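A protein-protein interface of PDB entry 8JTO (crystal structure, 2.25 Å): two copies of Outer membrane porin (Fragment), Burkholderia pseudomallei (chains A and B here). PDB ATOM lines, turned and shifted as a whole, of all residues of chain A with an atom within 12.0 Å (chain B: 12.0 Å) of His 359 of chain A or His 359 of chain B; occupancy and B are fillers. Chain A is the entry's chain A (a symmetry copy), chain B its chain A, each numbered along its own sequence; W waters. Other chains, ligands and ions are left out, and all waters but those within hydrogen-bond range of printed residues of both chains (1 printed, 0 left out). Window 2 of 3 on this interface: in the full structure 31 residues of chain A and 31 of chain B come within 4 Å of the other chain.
Hydrophobic or aromatic side chains of chain A within 4 Å of the printed part of chain B: Leu 6, His 356, His 358 and His 359. Along chain A the printed residues that touch a printed residue of chain B span positions 6 to 359. Of the 14 printed residues of chain B, 5 touch a printed residue of chain A. Hydrophobic or aromatic side chains of chain B within 4 Å of the printed part of chain A: Val 4, Leu 44, His 358 and His 359.
N of Ser 2 of chain B is in hydrogen-bond range of O of Ser 47 of chain B, 3.4 Å away. O of Val 4 of chain A is in hydrogen-bond range of ND1 of His 358 of chain A (2.8 Å). O of Leu 6 of chain A lies within hydrogen-bond range of N of His 356 of chain A (2.8 Å). ND1 of His 358 of chain B lies within hydrogen-bond range of O of Val 4 of chain B (2.8 Å).
N of Ser 2 of chain B sits close to NH1 of Arg 308 of chain A, at 2.8 Å. NE2 of His 356 of chain A is in hydrogen-bond range of O of His 358 of chain B, at 3.2 Å. NE2 of His 359 of chain A lies close to NE2 of His 359 of chain B.
Among the printed residues, merely in contact across the chains: His 356 of chain A with Val 4 of chain B (3.5 Å), His 358 of chain A with His 358 of chain B (3.6 Å) and Leu 6 of chain A with Leu 44 of chain B (3.999 Å).
Water W1 lies within hydrogen-bond range of O of His 357 of chain B, O of His 358 of chain B, N of Val 4 of chain B and NE2 of His 356 of chain A.
Leu 6 of chain A touches Leu 44 of chain B, but with the chains exchanged Leu 44 of chain A does not touch Leu 6 of chain B (9.3 Å). His 356 of chain A touches Val 4 of chain B, but with the chains exchanged Val 4 of chain A does not touch His 356 of chain B (12.6 Å). His 358 of chain B touches its own counterpart, His 358 of chain A. His 359 of chain A touches its own counterpart, His 359 of chain B. 14 positions are printed for both chains.
Ser 2 of chain A touches none of the printed residues of chain B. Arg 45 of chain A touches none of the printed residues of chain B. Of the printed residues of chain B, His 356 of chain A touches Val 4 (3.5 Å) and His 358 (3.2 Å). His 358 of chain A touches one residue of chain B. Printed residues of chain A within 4 Å of Ser 2 of chain B: Arg 308 (2.8 Å). Of the printed residues of chain A, Leu 44 of chain B touches Leu 6 (3.999 Å). His 358 of chain B touches just these residues of chain A: His 356 and His 358. Printed residues of chain A within 4 Å of His 359 of chain B: His 359.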
ATOM      1  N   SER A   2      12.950  10.629   8.802  1.00  0.00           N
ATOM      2  CA  SER A   2      14.365  10.677   8.471  1.00  0.00           C
ATOM      3  C   SER A   2      15.056   9.335   8.726  1.00  0.00           C
ATOM      4  O   SER A   2      16.236   9.177   8.400  1.00  0.00           O
ATOM      5  CB  SER A   2      15.054  11.789   9.265  1.00  0.00           C
ATOM      6  OG  SER A   2      14.328  13.005   9.144  1.00  0.00           O
ATOM      7  N   SER A   3      14.315   8.375   9.293  1.00  0.00           N
ATOM      8  CA  SER A   3      14.860   7.064   9.642  1.00  0.00           C
ATOM      9  C   SER A   3      13.797   6.142  10.225  1.00  0.00           C
ATOM     10  O   SER A   3      13.099   6.527  11.169  1.00  0.00           O
ATOM     11  CB  SER A   3      16.006   7.202  10.651  1.00  0.00           C
ATOM     12  OG  SER A   3      15.504   7.369  11.969  1.00  0.00           O
ATOM     13  N   VAL A   4      13.679   4.927   9.684  1.00  0.00           N
ATOM     14  CA  VAL A   4      12.814   3.881  10.225  1.00  0.00           C
ATOM     15  C   VAL A   4      13.634   2.607  10.390  1.00  0.00           C
ATOM     16  O   VAL A   4      14.216   2.113   9.419  1.00  0.00           O
ATOM     17  CB  VAL A   4      11.588   3.615   9.331  1.00  0.00           C
ATOM     18  CG1 VAL A   4      10.750   2.477   9.914  1.00  0.00           C
ATOM     19  CG2 VAL A   4      10.751   4.880   9.198  1.00  0.00           C
ATOM     20  N   THR A   5      13.668   2.073  11.611  1.00  0.00           N
ATOM     21  CA  THR A   5      14.508   0.929  11.950  1.00  0.00           C
ATOM     22  C   THR A   5      13.651  -0.282  12.289  1.00  0.00           C
ATOM     23  O   THR A   5      12.722  -0.190  13.101  1.00  0.00           O
ATOM     24  CB  THR A   5      15.436   1.243  13.132  1.00  0.00           C
ATOM     25  OG1 THR A   5      16.245   2.380  12.824  1.00  0.00           O
ATOM     26  CG2 THR A   5      16.334   0.055  13.438  1.00  0.00           C
ATOM     27  N   LEU A   6      13.966  -1.409  11.667  1.00  0.00           N
ATOM     28  CA  LEU A   6      13.416  -2.698  12.050  1.00  0.00           C
ATOM     29  C   LEU A   6      14.433  -3.394  12.943  1.00  0.00           C
ATOM     30  O   LEU A   6      15.635  -3.359  12.670  1.00  0.00           O
ATOM     31  CB  LEU A   6      13.103  -3.554  10.818  1.00  0.00           C
ATOM     32  CG  LEU A   6      13.047  -5.073  11.016  1.00  0.00           C
ATOM     33  CD1 LEU A   6      11.691  -5.509  11.582  1.00  0.00           C
ATOM     34  CD2 LEU A   6      13.387  -5.822   9.716  1.00  0.00           C
ATOM     35  N   LEU A  44       9.395  -1.910  15.150  1.00  0.00           N
ATOM     36  CA  LEU A  44       9.646  -0.830  14.209  1.00  0.00           C
ATOM     37  C   LEU A  44       9.723   0.463  15.001  1.00  0.00           C
ATOM     38  O   LEU A  44       8.839   0.737  15.818  1.00  0.00           O
ATOM     39  CB  LEU A  44       8.530  -0.731  13.162  1.00  0.00           C
ATOM     40  CG  LEU A  44       8.613  -1.613  11.913  1.00  0.00           C
ATOM     41  CD1 LEU A  44       7.391  -1.391  11.019  1.00  0.00           C
ATOM     42  CD2 LEU A  44       9.905  -1.332  11.144  1.00  0.00           C
ATOM     43  N   ARG A  45      10.767   1.254  14.764  1.00  0.00           N
ATOM     44  CA  ARG A  45      10.911   2.544  15.422  1.00  0.00           C
ATOM     45  C   ARG A  45      11.405   3.561  14.408  1.00  0.00           C
ATOM     46  O   ARG A  45      12.085   3.216  13.438  1.00  0.00           O
ATOM     47  CB  ARG A  45      11.883   2.490  16.609  1.00  0.00           C
ATOM     48  CG  ARG A  45      13.279   2.048  16.231  1.00  0.00           C
ATOM     49  CD  ARG A  45      14.309   2.395  17.307  1.00  0.00           C
ATOM     50  NE  ARG A  45      14.468   1.285  18.237  1.00  0.00           N
ATOM     51  CZ  ARG A  45      15.628   0.737  18.574  1.00  0.00           C
ATOM     52  NH1 ARG A  45      16.772   1.172  18.071  1.00  0.00           N
ATOM     53  NH2 ARG A  45      15.638  -0.284  19.428  1.00  0.00           N
ATOM     54  N   GLY A  46      11.063   4.820  14.642  1.00  0.00           N
ATOM     55  CA  GLY A  46      11.496   5.864  13.734  1.00  0.00           C
ATOM     56  C   GLY A  46      11.493   7.218  14.397  1.00  0.00           C
ATOM     57  O   GLY A  46      10.857   7.429  15.436  1.00  0.00           O
ATOM     58  N   SER A  47      12.229   8.138  13.784  1.00  0.00           N
ATOM     59  CA  SER A  47      12.197   9.536  14.181  1.00  0.00           C
ATOM     60  C   SER A  47      12.397  10.396  12.943  1.00  0.00           C
ATOM     61  O   SER A  47      13.287  10.117  12.135  1.00  0.00           O
ATOM     62  CB  SER A  47      13.267   9.848  15.232  1.00  0.00           C
ATOM     63  OG  SER A  47      14.554   9.665  14.691  1.00  0.00           O
ATOM     64  N   ARG A 308      26.141  -8.809  18.342  1.00  0.00           N
ATOM     65  CA  ARG A 308      24.735  -9.178  18.235  1.00  0.00           C
ATOM     66  C   ARG A 308      24.364 -10.479  18.934  1.00  0.00           C
ATOM     67  O   ARG A 308      23.182 -10.681  19.225  1.00  0.00           O
ATOM     68  CB  ARG A 308      24.332  -9.293  16.760  1.00  0.00           C
ATOM     69  CG  ARG A 308      24.461  -7.990  15.992  1.00  0.00           C
ATOM     70  CD  ARG A 308      24.500  -8.258  14.501  1.00  0.00           C
ATOM     71  NE  ARG A 308      23.244  -8.844  14.049  1.00  0.00           N
ATOM     72  CZ  ARG A 308      23.048  -9.368  12.847  1.00  0.00           C
ATOM     73  NH1 ARG A 308      23.992  -9.335  11.919  1.00  0.00           N
ATOM     74  NH2 ARG A 308      21.877  -9.944  12.571  1.00  0.00           N
ATOM     75  N   HIS A 355      18.951  -5.911  13.427  1.00  0.00           N
ATOM     76  CA  HIS A 355      18.854  -4.466  13.287  1.00  0.00           C
ATOM     77  C   HIS A 355      18.999  -4.041  11.835  1.00  0.00           C
ATOM     78  O   HIS A 355      20.008  -4.363  11.205  1.00  0.00           O
ATOM     79  CB  HIS A 355      19.948  -3.807  14.118  1.00  0.00           C
ATOM     80  CG  HIS A 355      19.513  -2.563  14.811  1.00  0.00           C
ATOM     81  ND1 HIS A 355      18.375  -2.502  15.586  1.00  0.00           N
ATOM     82  CD2 HIS A 355      20.066  -1.330  14.853  1.00  0.00           C
ATOM     83  CE1 HIS A 355      18.246  -1.284  16.076  1.00  0.00           C
ATOM     84  NE2 HIS A 355      19.259  -0.552  15.645  1.00  0.00           N
ATOM     85  N   HIS A 356      18.027  -3.314  11.285  1.00  0.00           N
ATOM     86  CA  HIS A 356      18.211  -2.754   9.953  1.00  0.00           C
ATOM     87  C   HIS A 356      17.697  -1.324   9.883  1.00  0.00           C
ATOM     88  O   HIS A 356      16.532  -1.058  10.193  1.00  0.00           O
ATOM     89  CB  HIS A 356      17.556  -3.625   8.887  1.00  0.00           C
ATOM     90  CG  HIS A 356      18.548  -4.491   8.177  1.00  0.00           C
ATOM     91  ND1 HIS A 356      18.871  -5.762   8.606  1.00  0.00           N
ATOM     92  CD2 HIS A 356      19.371  -4.226   7.135  1.00  0.00           C
ATOM     93  CE1 HIS A 356      19.805  -6.264   7.821  1.00  0.00           C
ATOM     94  NE2 HIS A 356      20.128  -5.353   6.920  1.00  0.00           N
ATOM     95  N   HIS A 357      18.581  -0.417   9.452  1.00  0.00           N
ATOM     96  CA  HIS A 357      18.373   1.025   9.530  1.00  0.00           C
ATOM     97  C   HIS A 357      17.748   1.634   8.283  1.00  0.00           C
ATOM     98  O   HIS A 357      17.332   2.794   8.332  1.00  0.00           O
ATOM     99  CB  HIS A 357      19.703   1.726   9.806  1.00  0.00           C
ATOM    100  CG  HIS A 357      20.133   1.657  11.235  1.00  0.00           C
ATOM    101  ND1 HIS A 357      19.274   1.906  12.284  1.00  0.00           N
ATOM    102  CD2 HIS A 357      21.329   1.353  11.792  1.00  0.00           C
ATOM    103  CE1 HIS A 357      19.924   1.768  13.426  1.00  0.00           C
ATOM    104  NE2 HIS A 357      21.174   1.433  13.155  1.00  0.00           N
ATOM    105  N   HIS A 358      17.678   0.897   7.172  1.00  0.00           N
ATOM    106  CA  HIS A 358      17.008   1.362   5.955  1.00  0.00           C
ATOM    107  C   HIS A 358      17.604   2.687   5.466  1.00  0.00           C
ATOM    108  O   HIS A 358      16.969   3.745   5.499  1.00  0.00           O
ATOM    109  CB  HIS A 358      15.499   1.508   6.185  1.00  0.00           C
ATOM    110  CG  HIS A 358      14.796   0.215   6.447  1.00  0.00           C
ATOM    111  ND1 HIS A 358      14.087  -0.023   7.605  1.00  0.00           N
ATOM    112  CD2 HIS A 358      14.689  -0.908   5.701  1.00  0.00           C
ATOM    113  CE1 HIS A 358      13.574  -1.239   7.560  1.00  0.00           C
ATOM    114  NE2 HIS A 358      13.930  -1.798   6.420  1.00  0.00           N
ATOM    115  N   HIS A 359      18.846   2.598   5.001  1.00  0.00           N
ATOM    116  CA  HIS A 359      19.554   3.775   4.506  1.00  0.00           C
ATOM    117  C   HIS A 359      18.938   4.310   3.213  1.00  0.00           C
ATOM    118  O   HIS A 359      18.518   3.542   2.344  1.00  0.00           O
ATOM    119  CB  HIS A 359      21.028   3.455   4.284  1.00  0.00           C
ATOM    120  CG  HIS A 359      21.298   2.688   3.028  1.00  0.00           C
ATOM    121  ND1 HIS A 359      20.970   1.357   2.882  1.00  0.00           N
ATOM    122  CD2 HIS A 359      21.844   3.072   1.850  1.00  0.00           C
ATOM    123  CE1 HIS A 359      21.317   0.950   1.673  1.00  0.00           C
ATOM    124  NE2 HIS A 359      21.847   1.973   1.027  1.00  0.00           N
ATOM    125  N   SER B   2      24.989 -10.402   9.551  1.00  0.00           N
ATOM    126  CA  SER B   2      25.572 -10.109   8.251  1.00  0.00           C
ATOM    127  C   SER B   2      24.509 -10.024   7.154  1.00  0.00           C
ATOM    128  O   SER B   2      24.828  -9.683   6.012  1.00  0.00           O
ATOM    129  CB  SER B   2      26.620 -11.167   7.896  1.00  0.00           C
ATOM    130  OG  SER B   2      27.524 -11.349   8.977  1.00  0.00           O
ATOM    131  N   SER B   3      23.253 -10.321   7.510  1.00  0.00           N
ATOM    132  CA  SER B   3      22.148 -10.333   6.554  1.00  0.00           C
ATOM    133  C   SER B   3      20.817 -10.652   7.224  1.00  0.00           C
ATOM    134  O   SER B   3      20.713 -11.654   7.939  1.00  0.00           O
ATOM    135  CB  SER B   3      22.401 -11.357   5.441  1.00  0.00           C
ATOM    136  OG  SER B   3      22.070 -12.669   5.873  1.00  0.00           O
ATOM    137  N   VAL B   4      19.800  -9.818   6.989  1.00  0.00           N
ATOM    138  CA  VAL B   4      18.431 -10.068   7.436  1.00  0.00           C
ATOM    139  C   VAL B   4      17.494  -9.913   6.245  1.00  0.00           C
ATOM    140  O   VAL B   4      17.468  -8.855   5.607  1.00  0.00           O
ATOM    141  CB  VAL B   4      18.007  -9.121   8.574  1.00  0.00           C
ATOM    142  CG1 VAL B   4      16.552  -9.387   8.964  1.00  0.00           C
ATOM    143  CG2 VAL B   4      18.923  -9.303   9.777  1.00  0.00           C
ATOM    144  N   THR B   5      16.720 -10.960   5.954  1.00  0.00           N
ATOM    145  CA  THR B   5      15.865 -11.007   4.773  1.00  0.00           C
ATOM    146  C   THR B   5      14.397 -11.019   5.175  1.00  0.00           C
ATOM    147  O   THR B   5      13.982 -11.817   6.023  1.00  0.00           O
ATOM    148  CB  THR B   5      16.166 -12.241   3.910  1.00  0.00           C
ATOM    149  OG1 THR B   5      17.544 -12.241   3.528  1.00  0.00           O
ATOM    150  CG2 THR B   5      15.298 -12.246   2.661  1.00  0.00           C
ATOM    151  N   LEU B   6      13.620 -10.135   4.563  1.00  0.00           N
ATOM    152  CA  LEU B   6      12.171 -10.173   4.647  1.00  0.00           C
ATOM    153  C   LEU B   6      11.649 -10.872   3.401  1.00  0.00           C
ATOM    154  O   LEU B   6      12.138 -10.631   2.295  1.00  0.00           O
ATOM    155  CB  LEU B   6      11.587  -8.761   4.760  1.00  0.00           C
ATOM    156  CG  LEU B   6      10.133  -8.567   4.317  1.00  0.00           C
ATOM    157  CD1 LEU B   6       9.155  -8.988   5.420  1.00  0.00           C
ATOM    158  CD2 LEU B   6       9.874  -7.124   3.851  1.00  0.00           C
ATOM    159  N   LEU B  44      10.830 -13.326   8.476  1.00  0.00           N
ATOM    160  CA  LEU B  44      12.128 -12.691   8.650  1.00  0.00           C
ATOM    161  C   LEU B  44      13.141 -13.786   8.930  1.00  0.00           C
ATOM    162  O   LEU B  44      12.906 -14.636   9.794  1.00  0.00           O
ATOM    163  CB  LEU B  44      12.109 -11.691   9.812  1.00  0.00           C
ATOM    164  CG  LEU B  44      11.635 -10.260   9.544  1.00  0.00           C
ATOM    165  CD1 LEU B  44      11.657  -9.437  10.834  1.00  0.00           C
ATOM    166  CD2 LEU B  44      12.498  -9.602   8.465  1.00  0.00           C
ATOM    167  N   ARG B  45      14.261 -13.769   8.211  1.00  0.00           N
ATOM    168  CA  ARG B  45      15.327 -14.734   8.438  1.00  0.00           C
ATOM    169  C   ARG B  45      16.664 -14.016   8.365  1.00  0.00           C
ATOM    170  O   ARG B  45      16.805 -12.999   7.683  1.00  0.00           O
ATOM    171  CB  ARG B  45      15.305 -15.880   7.416  1.00  0.00           C
ATOM    172  CG  ARG B  45      15.447 -15.418   5.983  1.00  0.00           C
ATOM    173  CD  ARG B  45      15.838 -16.558   5.042  1.00  0.00           C
ATOM    174  NE  ARG B  45      14.648 -17.178   4.472  1.00  0.00           N
ATOM    175  CZ  ARG B  45      14.443 -17.380   3.177  1.00  0.00           C
ATOM    176  NH1 ARG B  45      15.335 -17.016   2.270  1.00  0.00           N
ATOM    177  NH2 ARG B  45      13.306 -17.947   2.782  1.00  0.00           N
ATOM    178  N   GLY B  46      17.646 -14.557   9.072  1.00  0.00           N
ATOM    179  CA  GLY B  46      18.962 -13.949   9.059  1.00  0.00           C
ATOM    180  C   GLY B  46      20.037 -14.933   9.443  1.00  0.00           C
ATOM    181  O   GLY B  46      19.771 -15.983  10.038  1.00  0.00           O
ATOM    182  N   SER B  47      21.266 -14.581   9.083  1.00  0.00           N
ATOM    183  CA  SER B  47      22.437 -15.319   9.529  1.00  0.00           C
ATOM    184  C   SER B  47      23.589 -14.341   9.702  1.00  0.00           C
ATOM    185  O   SER B  47      23.820 -13.499   8.830  1.00  0.00           O
ATOM    186  CB  SER B  47      22.814 -16.427   8.541  1.00  0.00           C
ATOM    187  OG  SER B  47      23.198 -15.872   7.305  1.00  0.00           O
ATOM    188  N   HIS B 355      10.700 -10.754  -1.705  1.00  0.00           N
ATOM    189  CA  HIS B 355      12.023 -10.984  -1.145  1.00  0.00           C
ATOM    190  C   HIS B 355      12.812  -9.689  -1.043  1.00  0.00           C
ATOM    191  O   HIS B 355      12.998  -9.010  -2.054  1.00  0.00           O
ATOM    192  CB  HIS B 355      12.779 -11.967  -2.030  1.00  0.00           C
ATOM    193  CG  HIS B 355      13.606 -12.948  -1.274  1.00  0.00           C
ATOM    194  ND1 HIS B 355      13.103 -13.700  -0.234  1.00  0.00           N
ATOM    195  CD2 HIS B 355      14.903 -13.307  -1.408  1.00  0.00           C
ATOM    196  CE1 HIS B 355      14.056 -14.481   0.240  1.00  0.00           C
ATOM    197  NE2 HIS B 355      15.159 -14.261  -0.454  1.00  0.00           N
ATOM    198  N   HIS B 356      13.294  -9.329   0.147  1.00  0.00           N
ATOM    199  CA  HIS B 356      14.190  -8.185   0.246  1.00  0.00           C
ATOM    200  C   HIS B 356      15.346  -8.474   1.191  1.00  0.00           C
ATOM    201  O   HIS B 356      15.134  -8.827   2.355  1.00  0.00           O
ATOM    202  CB  HIS B 356      13.439  -6.926   0.666  1.00  0.00           C
ATOM    203  CG  HIS B 356      13.143  -6.031  -0.496  1.00  0.00           C
ATOM    204  ND1 HIS B 356      11.983  -6.128  -1.235  1.00  0.00           N
ATOM    205  CD2 HIS B 356      13.906  -5.100  -1.115  1.00  0.00           C
ATOM    206  CE1 HIS B 356      12.018  -5.252  -2.222  1.00  0.00           C
ATOM    207  NE2 HIS B 356      13.175  -4.614  -2.173  1.00  0.00           N
ATOM    208  N   HIS B 357      16.568  -8.297   0.674  1.00  0.00           N
ATOM    209  CA  HIS B 357      17.798  -8.735   1.323  1.00  0.00           C
ATOM    210  C   HIS B 357      18.454  -7.676   2.197  1.00  0.00           C
ATOM    211  O   HIS B 357      19.368  -8.012   2.955  1.00  0.00           O
ATOM    212  CB  HIS B 357      18.804  -9.194   0.268  1.00  0.00           C
ATOM    213  CG  HIS B 357      18.534 -10.565  -0.264  1.00  0.00           C
ATOM    214  ND1 HIS B 357      18.227 -11.632   0.553  1.00  0.00           N
ATOM    215  CD2 HIS B 357      18.510 -11.040  -1.531  1.00  0.00           C
ATOM    216  CE1 HIS B 357      18.034 -12.709  -0.189  1.00  0.00           C
ATOM    217  NE2 HIS B 357      18.201 -12.377  -1.457  1.00  0.00           N
ATOM    218  N   HIS B 358      18.029  -6.415   2.109  1.00  0.00           N
ATOM    219  CA  HIS B 358      18.532  -5.347   2.977  1.00  0.00           C
ATOM    220  C   HIS B 358      20.055  -5.216   2.869  1.00  0.00           C
ATOM    221  O   HIS B 358      20.808  -5.509   3.803  1.00  0.00           O
ATOM    222  CB  HIS B 358      18.118  -5.588   4.434  1.00  0.00           C
ATOM    223  CG  HIS B 358      16.645  -5.507   4.670  1.00  0.00           C
ATOM    224  ND1 HIS B 358      15.915  -6.559   5.181  1.00  0.00           N
ATOM    225  CD2 HIS B 358      15.765  -4.500   4.468  1.00  0.00           C
ATOM    226  CE1 HIS B 358      14.647  -6.201   5.284  1.00  0.00           C
ATOM    227  NE2 HIS B 358      14.530  -4.961   4.852  1.00  0.00           N
ATOM    228  N   HIS B 359      20.491  -4.758   1.700  1.00  0.00           N
ATOM    229  CA  HIS B 359      21.917  -4.585   1.439  1.00  0.00           C
ATOM    230  C   HIS B 359      22.520  -3.462   2.286  1.00  0.00           C
ATOM    231  O   HIS B 359      21.893  -2.423   2.501  1.00  0.00           O
ATOM    232  CB  HIS B 359      22.157  -4.307  -0.040  1.00  0.00           C
ATOM    233  CG  HIS B 359      21.850  -2.900  -0.447  1.00  0.00           C
ATOM    234  ND1 HIS B 359      20.562  -2.418  -0.550  1.00  0.00           N
ATOM    235  CD2 HIS B 359      22.665  -1.864  -0.758  1.00  0.00           C
ATOM    236  CE1 HIS B 359      20.598  -1.150  -0.920  1.00  0.00           C
ATOM    237  NE2 HIS B 359      21.861  -0.790  -1.050  1.00  0.00           N
HETATM  238  O   HOH W   1      20.903  -7.805   5.029  1.00  0.00           O
